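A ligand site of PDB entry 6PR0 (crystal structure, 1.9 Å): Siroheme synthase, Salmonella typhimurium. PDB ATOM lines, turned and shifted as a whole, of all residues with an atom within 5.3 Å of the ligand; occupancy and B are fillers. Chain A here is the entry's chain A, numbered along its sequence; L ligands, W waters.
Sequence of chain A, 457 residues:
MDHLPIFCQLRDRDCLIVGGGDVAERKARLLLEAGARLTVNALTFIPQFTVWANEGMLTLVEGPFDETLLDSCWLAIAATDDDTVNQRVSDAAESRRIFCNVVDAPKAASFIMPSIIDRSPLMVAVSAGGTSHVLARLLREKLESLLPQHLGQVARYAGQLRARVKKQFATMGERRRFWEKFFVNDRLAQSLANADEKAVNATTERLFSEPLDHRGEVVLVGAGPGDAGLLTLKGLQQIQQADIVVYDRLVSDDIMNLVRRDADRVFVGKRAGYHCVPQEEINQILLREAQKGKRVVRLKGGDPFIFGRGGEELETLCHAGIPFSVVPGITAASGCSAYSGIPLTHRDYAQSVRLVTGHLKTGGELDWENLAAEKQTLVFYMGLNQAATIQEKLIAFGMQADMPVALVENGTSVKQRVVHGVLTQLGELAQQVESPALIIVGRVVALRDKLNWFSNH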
ATOM      1  N   PRO A 225     -13.232   7.431 -28.598  1.00  0.00           N
ATOM      2  CA  PRO A 225     -14.221   6.359 -28.393  1.00  0.00           C
ATOM      3  C   PRO A 225     -14.257   5.327 -29.507  1.00  0.00           C
ATOM      4  O   PRO A 225     -14.916   4.299 -29.344  1.00  0.00           O
ATOM      5  CB  PRO A 225     -15.557   7.114 -28.285  1.00  0.00           C
ATOM      6  CG  PRO A 225     -15.337   8.401 -28.925  1.00  0.00           C
ATOM      7  CD  PRO A 225     -13.851   8.693 -29.031  1.00  0.00           C
ATOM      8  N   GLY A 226     -13.581   5.541 -30.626  1.00  0.00           N
ATOM      9  CA  GLY A 226     -13.523   4.470 -31.617  1.00  0.00           C
ATOM     10  C   GLY A 226     -13.124   4.917 -33.008  1.00  0.00           C
ATOM     11  O   GLY A 226     -12.201   4.342 -33.595  1.00  0.00           O
ATOM     12  N   LEU A 250     -11.132  -1.565 -25.546  1.00  0.00           N
ATOM     13  CA  LEU A 250     -11.878  -0.388 -25.980  1.00  0.00           C
ATOM     14  C   LEU A 250     -11.070   0.526 -26.893  1.00  0.00           C
ATOM     15  O   LEU A 250     -11.523   1.624 -27.216  1.00  0.00           O
ATOM     16  CB  LEU A 250     -12.408   0.371 -24.760  1.00  0.00           C
ATOM     17  CG  LEU A 250     -13.598  -0.413 -24.161  1.00  0.00           C
ATOM     18  CD1 LEU A 250     -14.557   0.476 -23.384  1.00  0.00           C
ATOM     19  CD2 LEU A 250     -14.375  -1.127 -25.286  1.00  0.00           C
ATOM     20  N   GLY A 301      -8.950   3.625 -24.214  1.00  0.00           N
ATOM     21  CA  GLY A 301     -10.171   4.103 -24.836  1.00  0.00           C
ATOM     22  C   GLY A 301     -10.607   5.442 -24.276  1.00  0.00           C
ATOM     23  O   GLY A 301     -10.444   5.733 -23.088  1.00  0.00           O
ATOM     24  N   GLY A 302     -11.134   6.312 -25.159  1.00  0.00           N
ATOM     25  CA  GLY A 302     -11.690   7.562 -24.667  1.00  0.00           C
ATOM     26  C   GLY A 302     -10.592   8.494 -24.186  1.00  0.00           C
ATOM     27  O   GLY A 302      -9.571   8.682 -24.854  1.00  0.00           O
ATOM     28  N   ASP A 303     -10.793   9.099 -23.018  1.00  0.00           N
ATOM     29  CA  ASP A 303      -9.816   9.961 -22.358  1.00  0.00           C
ATOM     30  C   ASP A 303      -9.160   9.227 -21.176  1.00  0.00           C
ATOM     31  O   ASP A 303      -9.836   8.532 -20.429  1.00  0.00           O
ATOM     32  CB  ASP A 303     -10.481  11.224 -21.850  1.00  0.00           C
ATOM     33  CG  ASP A 303      -9.496  12.178 -21.180  1.00  0.00           C
ATOM     34  OD1 ASP A 303      -8.868  12.995 -21.890  1.00  0.00           O
ATOM     35  OD2 ASP A 303      -9.318  12.061 -19.951  1.00  0.00           O
ATOM     36  N   PRO A 304      -7.850   9.398 -20.957  1.00  0.00           N
ATOM     37  CA  PRO A 304      -7.158   8.597 -19.930  1.00  0.00           C
ATOM     38  C   PRO A 304      -7.599   8.909 -18.499  1.00  0.00           C
ATOM     39  O   PRO A 304      -7.494   8.039 -17.633  1.00  0.00           O
ATOM     40  CB  PRO A 304      -5.668   8.935 -20.135  1.00  0.00           C
ATOM     41  CG  PRO A 304      -5.594   9.545 -21.511  1.00  0.00           C
ATOM     42  CD  PRO A 304      -6.922  10.227 -21.754  1.00  0.00           C
ATOM     43  N   ILE A 306     -10.656   9.972 -17.283  1.00  0.00           N
ATOM     44  CA  ILE A 306     -12.098   9.881 -16.960  1.00  0.00           C
ATOM     45  C   ILE A 306     -12.441   8.396 -16.882  1.00  0.00           C
ATOM     46  O   ILE A 306     -12.584   7.723 -17.914  1.00  0.00           O
ATOM     47  CB  ILE A 306     -12.960  10.622 -18.000  1.00  0.00           C
ATOM     48  CG1 ILE A 306     -12.714  12.134 -17.912  1.00  0.00           C
ATOM     49  CG2 ILE A 306     -14.468  10.272 -17.835  1.00  0.00           C
ATOM     50  CD1 ILE A 306     -13.264  12.925 -19.090  1.00  0.00           C
ATOM     51  N   PHE A 307     -12.539   7.886 -15.648  1.00  0.00           N
ATOM     52  CA  PHE A 307     -12.848   6.477 -15.371  1.00  0.00           C
ATOM     53  C   PHE A 307     -11.934   5.527 -16.150  1.00  0.00           C
ATOM     54  O   PHE A 307     -12.347   4.450 -16.586  1.00  0.00           O
ATOM     55  CB  PHE A 307     -14.322   6.171 -15.658  1.00  0.00           C
ATOM     56  CG  PHE A 307     -15.282   7.046 -14.882  1.00  0.00           C
ATOM     57  CD1 PHE A 307     -15.314   7.001 -13.500  1.00  0.00           C
ATOM     58  CD2 PHE A 307     -16.140   7.920 -15.533  1.00  0.00           C
ATOM     59  CE1 PHE A 307     -16.187   7.808 -12.780  1.00  0.00           C
ATOM     60  CE2 PHE A 307     -17.013   8.728 -14.814  1.00  0.00           C
ATOM     61  CZ  PHE A 307     -17.029   8.676 -13.456  1.00  0.00           C
ATOM     62  N   GLY A 308     -10.680   5.929 -16.326  1.00  0.00           N
ATOM     63  CA  GLY A 308      -9.711   5.115 -17.022  1.00  0.00           C
ATOM     64  C   GLY A 308      -8.584   4.597 -16.146  1.00  0.00           C
ATOM     65  O   GLY A 308      -7.696   3.901 -16.668  1.00  0.00           O
ATOM     66  N   ILE A 330     -10.817  12.197 -26.750  1.00  0.00           N
ATOM     67  CA  ILE A 330     -12.266  12.439 -26.761  1.00  0.00           C
ATOM     68  C   ILE A 330     -12.939  11.389 -25.852  1.00  0.00           C
ATOM     69  O   ILE A 330     -12.928  10.196 -26.176  1.00  0.00           O
ATOM     70  CB  ILE A 330     -12.831  12.374 -28.183  1.00  0.00           C
ATOM     71  CG1 ILE A 330     -12.038  13.256 -29.160  1.00  0.00           C
ATOM     72  CG2 ILE A 330     -14.373  12.663 -28.159  1.00  0.00           C
ATOM     73  CD1 ILE A 330     -12.252  14.738 -29.012  1.00  0.00           C
ATOM     74  N   THR A 331     -13.541  11.824 -24.744  1.00  0.00           N
ATOM     75  CA  THR A 331     -14.207  10.861 -23.875  1.00  0.00           C
ATOM     76  C   THR A 331     -15.484  10.374 -24.557  1.00  0.00           C
ATOM     77  O   THR A 331     -16.017  11.010 -25.458  1.00  0.00           O
ATOM     78  CB  THR A 331     -14.511  11.494 -22.512  1.00  0.00           C
ATOM     79  OG1 THR A 331     -14.922  10.484 -21.581  1.00  0.00           O
ATOM     80  CG2 THR A 331     -15.582  12.560 -22.649  1.00  0.00           C
ATOM     81  N   ALA A 332     -15.948   9.189 -24.145  1.00  0.00           N
ATOM     82  CA  ALA A 332     -17.171   8.616 -24.734  1.00  0.00           C
ATOM     83  C   ALA A 332     -18.329   9.612 -24.727  1.00  0.00           C
ATOM     84  O   ALA A 332     -19.112   9.664 -25.688  1.00  0.00           O
ATOM     85  CB  ALA A 332     -17.589   7.358 -23.973  1.00  0.00           C
ATOM     86  N   ALA A 333     -18.488  10.374 -23.646  1.00  0.00           N
ATOM     87  CA  ALA A 333     -19.594  11.342 -23.572  1.00  0.00           C
ATOM     88  C   ALA A 333     -19.571  12.316 -24.746  1.00  0.00           C
ATOM     89  O   ALA A 333     -20.578  12.499 -25.439  1.00  0.00           O
ATOM     90  CB  ALA A 333     -19.540  12.109 -22.244  1.00  0.00           C
ATOM     91  N   CYS A 336     -20.014  10.241 -28.259  1.00  0.00           N
ATOM     92  CA  CYS A 336     -21.389   9.768 -28.415  1.00  0.00           C
ATOM     93  C   CYS A 336     -22.379  10.915 -28.579  1.00  0.00           C
ATOM     94  O   CYS A 336     -23.347  10.794 -29.346  1.00  0.00           O
ATOM     95  CB  CYS A 336     -21.811   8.911 -27.222  1.00  0.00           C
ATOM     96  SG  CYS A 336     -20.975   7.325 -27.195  1.00  0.00           S
ATOM     97  N   PHE A 380     -24.090   8.023 -17.868  1.00  0.00           N
ATOM     98  CA  PHE A 380     -23.597   6.912 -17.085  1.00  0.00           C
ATOM     99  C   PHE A 380     -22.628   6.096 -17.932  1.00  0.00           C
ATOM    100  O   PHE A 380     -22.985   5.615 -19.019  1.00  0.00           O
ATOM    101  CB  PHE A 380     -24.724   6.000 -16.592  1.00  0.00           C
ATOM    102  CG  PHE A 380     -25.658   6.646 -15.623  1.00  0.00           C
ATOM    103  CD1 PHE A 380     -26.782   7.331 -16.072  1.00  0.00           C
ATOM    104  CD2 PHE A 380     -25.430   6.549 -14.258  1.00  0.00           C
ATOM    105  CE1 PHE A 380     -27.662   7.919 -15.175  1.00  0.00           C
ATOM    106  CE2 PHE A 380     -26.299   7.144 -13.356  1.00  0.00           C
ATOM    107  CZ  PHE A 380     -27.414   7.836 -13.814  1.00  0.00           C
ATOM    108  N   TYR A 381     -21.431   5.921 -17.420  1.00  0.00           N
ATOM    109  CA  TYR A 381     -20.443   5.016 -17.994  1.00  0.00           C
ATOM    110  C   TYR A 381     -20.574   3.664 -17.302  1.00  0.00           C
ATOM    111  O   TYR A 381     -20.858   3.599 -16.102  1.00  0.00           O
ATOM    112  CB  TYR A 381     -19.036   5.569 -17.753  1.00  0.00           C
ATOM    113  CG  TYR A 381     -18.624   6.788 -18.587  1.00  0.00           C
ATOM    114  CD1 TYR A 381     -19.290   8.003 -18.479  1.00  0.00           C
ATOM    115  CD2 TYR A 381     -17.535   6.702 -19.449  1.00  0.00           C
ATOM    116  CE1 TYR A 381     -18.882   9.128 -19.252  1.00  0.00           C
ATOM    117  CE2 TYR A 381     -17.126   7.798 -20.209  1.00  0.00           C
ATOM    118  CZ  TYR A 381     -17.804   9.007 -20.106  1.00  0.00           C
ATOM    119  OH  TYR A 381     -17.366  10.087 -20.873  1.00  0.00           O
ATOM    120  N   MET A 382     -20.317   2.592 -18.065  1.00  0.00           N
ATOM    121  CA  MET A 382     -20.419   1.185 -17.620  1.00  0.00           C
ATOM    122  C   MET A 382     -21.617   0.956 -16.702  1.00  0.00           C
ATOM    123  O   MET A 382     -21.507   0.409 -15.597  1.00  0.00           O
ATOM    124  CB  MET A 382     -19.120   0.693 -16.964  1.00  0.00           C
ATOM    125  CG  MET A 382     -18.208   1.692 -16.263  1.00  0.00           C
ATOM    126  SD  MET A 382     -16.689   0.849 -15.683  1.00  0.00           S
ATOM    127  CE  MET A 382     -15.608   2.228 -15.363  1.00  0.00           C
ATOM    128  N   GLY A 383     -22.794   1.362 -17.185  1.00  0.00           N
ATOM    129  CA  GLY A 383     -23.998   1.266 -16.389  1.00  0.00           C
ATOM    130  C   GLY A 383     -25.039   0.311 -16.932  1.00  0.00           C
ATOM    131  O   GLY A 383     -26.140   0.218 -16.387  1.00  0.00           O
ATOM    132  N   VAL A 408     -26.338   4.814 -26.395  1.00  0.00           N
ATOM    133  CA  VAL A 408     -25.492   4.828 -27.579  1.00  0.00           C
ATOM    134  C   VAL A 408     -24.529   3.655 -27.440  1.00  0.00           C
ATOM    135  O   VAL A 408     -23.721   3.609 -26.506  1.00  0.00           O
ATOM    136  CB  VAL A 408     -24.743   6.161 -27.730  1.00  0.00           C
ATOM    137  CG1 VAL A 408     -23.965   6.199 -29.058  1.00  0.00           C
ATOM    138  CG2 VAL A 408     -25.722   7.334 -27.642  1.00  0.00           C
ATOM    139  N   GLU A 409     -24.626   2.712 -28.372  1.00  0.00           N
ATOM    140  CA  GLU A 409     -23.788   1.525 -28.397  1.00  0.00           C
ATOM    141  C   GLU A 409     -22.715   1.689 -29.460  1.00  0.00           C
ATOM    142  O   GLU A 409     -23.024   1.974 -30.618  1.00  0.00           O
ATOM    143  CB  GLU A 409     -24.641   0.293 -28.690  1.00  0.00           C
ATOM    144  CG  GLU A 409     -23.902  -1.006 -28.766  1.00  0.00           C
ATOM    145  CD  GLU A 409     -24.772  -2.120 -29.330  1.00  0.00           C
ATOM    146  OE1 GLU A 409     -25.250  -1.981 -30.477  1.00  0.00           O
ATOM    147  OE2 GLU A 409     -25.031  -3.103 -28.615  1.00  0.00           O
ATOM    148  N   ASN A 410     -21.456   1.473 -29.078  1.00  0.00           N
ATOM    149  CA  ASN A 410     -20.347   1.623 -30.011  1.00  0.00           C
ATOM    150  C   ASN A 410     -20.372   2.998 -30.671  1.00  0.00           C
ATOM    151  O   ASN A 410     -20.252   3.130 -31.893  1.00  0.00           O
ATOM    152  CB  ASN A 410     -20.365   0.517 -31.061  1.00  0.00           C
ATOM    153  CG  ASN A 410     -19.872  -0.805 -30.527  1.00  0.00           C
ATOM    154  OD1 ASN A 410     -18.791  -0.875 -29.957  1.00  0.00           O
ATOM    155  ND2 ASN A 410     -20.670  -1.853 -30.697  1.00  0.00           N
ATOM    156  N   GLY A 411     -20.505   4.038 -29.840  1.00  0.00           N
ATOM    157  CA  GLY A 411     -20.586   5.389 -30.367  1.00  0.00           C
ATOM    158  C   GLY A 411     -19.376   5.742 -31.209  1.00  0.00           C
ATOM    159  O   GLY A 411     -18.248   5.381 -30.881  1.00  0.00           O
ATOM    160  N   THR A 412     -19.626   6.482 -32.305  1.00  0.00           N
ATOM    161  CA  THR A 412     -18.663   6.991 -33.299  1.00  0.00           C
ATOM    162  C   THR A 412     -18.136   5.917 -34.238  1.00  0.00           C
ATOM    163  O   THR A 412     -17.447   6.237 -35.224  1.00  0.00           O
ATOM    164  CB  THR A 412     -17.474   7.742 -32.672  1.00  0.00           C
ATOM    165  OG1 THR A 412     -16.404   6.849 -32.281  1.00  0.00           O
ATOM    166  CG2 THR A 412     -17.909   8.651 -31.478  1.00  0.00           C
ATOM    167  N   PRO A 436     -19.631  -1.858 -25.570  1.00  0.00           N
ATOM    168  CA  PRO A 436     -19.672  -0.655 -24.734  1.00  0.00           C
ATOM    169  C   PRO A 436     -20.828   0.263 -25.100  1.00  0.00           C
ATOM    170  O   PRO A 436     -21.058   0.544 -26.274  1.00  0.00           O
ATOM    171  CB  PRO A 436     -18.337   0.017 -25.042  1.00  0.00           C
ATOM    172  CG  PRO A 436     -18.095  -0.332 -26.487  1.00  0.00           C
ATOM    173  CD  PRO A 436     -18.661  -1.721 -26.678  1.00  0.00           C
ATOM    174  N   ALA A 437     -21.516   0.764 -24.087  1.00  0.00           N
ATOM    175  CA  ALA A 437     -22.669   1.612 -24.320  1.00  0.00           C
ATOM    176  C   ALA A 437     -22.735   2.665 -23.213  1.00  0.00           C
ATOM    177  O   ALA A 437     -22.357   2.405 -22.067  1.00  0.00           O
ATOM    178  CB  ALA A 437     -23.962   0.804 -24.380  1.00  0.00           C
ATOM    179  N   LEU A 438     -23.214   3.838 -23.584  1.00  0.00           N
ATOM    180  CA  LEU A 438     -23.392   4.985 -22.703  1.00  0.00           C
ATOM    181  C   LEU A 438     -24.891   5.200 -22.496  1.00  0.00           C
ATOM    182  O   LEU A 438     -25.670   5.045 -23.433  1.00  0.00           O
ATOM    183  CB  LEU A 438     -22.790   6.234 -23.363  1.00  0.00           C
ATOM    184  CG  LEU A 438     -21.990   7.244 -22.560  1.00  0.00           C
ATOM    185  CD1 LEU A 438     -20.903   6.562 -21.785  1.00  0.00           C
ATOM    186  CD2 LEU A 438     -21.428   8.294 -23.512  1.00  0.00           C
HETATM  187  N1  LIG L   1     -11.850   6.508 -20.330  1.00  0.00           N
HETATM  188  C1  LIG L   1     -12.983   6.168 -21.199  1.00  0.00           C
HETATM  189  C2  LIG L   1     -14.033   5.326 -20.444  1.00  0.00           C
HETATM  190  C3  LIG L   1     -13.557   3.996 -19.841  1.00  0.00           C
HETATM  191  S1  LIG L   1     -14.874   3.294 -18.773  1.00  0.00           S
HETATM  192  C4  LIG L   1     -13.653   7.437 -21.737  1.00  0.00           C
HETATM  193  O1  LIG L   1     -13.211   8.546 -21.421  1.00  0.00           O
HETATM  194  O2  LIG L   1     -14.635   7.381 -22.491  1.00  0.00           O
HETATM  195  C5  LIG L   1     -15.667   2.288 -20.054  1.00  0.00           C
HETATM  196  C6  LIG L   1     -17.075   2.769 -20.436  1.00  0.00           C
HETATM  197  O3  LIG L   1     -17.038   3.853 -21.369  1.00  0.00           O
HETATM  198  C7  LIG L   1     -17.895   1.701 -21.167  1.00  0.00           C
HETATM  199  O4  LIG L   1     -18.493   0.790 -20.280  1.00  0.00           O
HETATM  200  C8  LIG L   1     -18.928   2.513 -21.909  1.00  0.00           C
HETATM  201  O5  LIG L   1     -19.940   2.925 -21.010  1.00  0.00           O
HETATM  202  C9  LIG L   1     -18.152   3.753 -22.258  1.00  0.00           C
HETATM  203  N2  LIG L   1     -17.697   3.765 -23.661  1.00  0.00           N
HETATM  204  C10 LIG L   1     -16.398   3.735 -24.100  1.00  0.00           C
HETATM  205  N3  LIG L   1     -16.400   3.802 -25.453  1.00  0.00           N
HETATM  206  C11 LIG L   1     -17.687   3.865 -25.881  1.00  0.00           C
HETATM  207  C12 LIG L   1     -18.255   3.937 -27.151  1.00  0.00           C
HETATM  208  N4  LIG L   1     -17.498   3.954 -28.274  1.00  0.00           N
HETATM  209  N5  LIG L   1     -19.631   4.008 -27.257  1.00  0.00           N
HETATM  210  C13 LIG L   1     -20.430   3.980 -26.141  1.00  0.00           C
HETATM  211  N6  LIG L   1     -19.876   3.917 -24.890  1.00  0.00           N
HETATM  212  C14 LIG L   1     -18.515   3.853 -24.758  1.00  0.00           C
HETATM  213  O   HOH W   1     -10.035   4.469 -20.643  1.00  0.00           O
HETATM  214  O   HOH W   2     -13.582   3.529 -26.147  1.00  0.00           O
HETATM  215  O   HOH W   3     -13.287   3.446 -23.077  1.00  0.00           O
HETATM  216  O   HOH W   4     -20.720  -0.604 -21.421  1.00  0.00           O
HETATM  217  O   HOH W   5     -17.123  -1.449 -20.920  1.00  0.00           O
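A nitrogen (N4) of the ligand sits at hydrogen-bond distance from the backbone carbonyl oxygen (O) of Gly 411, 3.1 Å away. The side-chain hydroxyl of Thr 331 is in hydrogen-bond range of an oxygen (O1) of the ligand. N of Asp 303 sits at hydrogen-bond distance from O1 of the ligand, 3.0 Å away. A nitrogen (N5) of the ligand lies close to the side-chain sulfur (SG) of Cys 336 (3.6 Å). The backbone carbonyl oxygen (O) of Ile 306 is in hydrogen-bond range of a nitrogen (N1) of the ligand (2.8 Å). A nitrogen (N1) of the ligand lies within hydrogen-bond range of the backbone carbonyl oxygen (O) of Asp 303 (2.9 Å). The backbone NH (N) of Ala 332 is in hydrogen-bond range of an oxygen (O2) of the ligand (2.8 Å). The backbone NH of Gly 411 lies within hydrogen-bond range of a nitrogen (N5) of the ligand, 2.7 Å away. An oxygen (O5) of the ligand sits at hydrogen-bond distance from the backbone NH (N) of Met 382, at 3.0 Å. A nitrogen (N1) of the ligand sits at hydrogen-bond distance from the backbone carbonyl oxygen of Gly 301. A nitrogen (N4) of the ligand is in hydrogen-bond range of the backbone carbonyl oxygen (O) of Pro 225, 2.8 Å away. An oxygen (O5) of the ligand is in hydrogen-bond range of the backbone carbonyl oxygen (O) of Ala 437 (2.7 Å).
The backbone carbonyl oxygen (O) of Ala 332 lies close to the side-chain sulfur (SG) of Cys 336. O of Pro 436 is in hydrogen-bond range of N of Asn 410 (3.0 Å). The side-chain hydroxyl (OH) of Tyr 381 sits at hydrogen-bond distance from the side-chain hydroxyl (OG1) of Thr 331 (2.6 Å). The backbone carbonyl oxygen (O) of Val 408 sits at hydrogen-bond distance from the backbone NH (N) of Leu 438 (3.0 Å). The side-chain hydroxyl of Tyr 381 sits at hydrogen-bond distance from the backbone NH of Ala 333 (3.0 Å).
The backbone carbonyl oxygen (O) of Phe 307 lies close to a sulfur (S1) of the ligand. Residues that only touch the ligand: Val 408 (3.3 Å), Tyr 381 (3.4 Å), Pro 436 (3.5 Å), Gly 302 (3.5 Å), Leu 438 (3.6 Å), Asn 410 (3.6 Å) and Leu 250 (3.8 Å). The nearest printed residue that does not touch the ligand is Gly 308 (4.2 Å).
Water W1 bridges a nitrogen (N1) of the ligand (2.7 Å) and the backbone carbonyl oxygen (O) of Gly 301 (2.8 Å). Water W4 lies within hydrogen-bond range of an oxygen (O4) of the ligand and the backbone NH (N) of Ala 437. Water W2 bridges N3 of the ligand (2.9 Å) and O of Leu 250 (3.0 Å).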
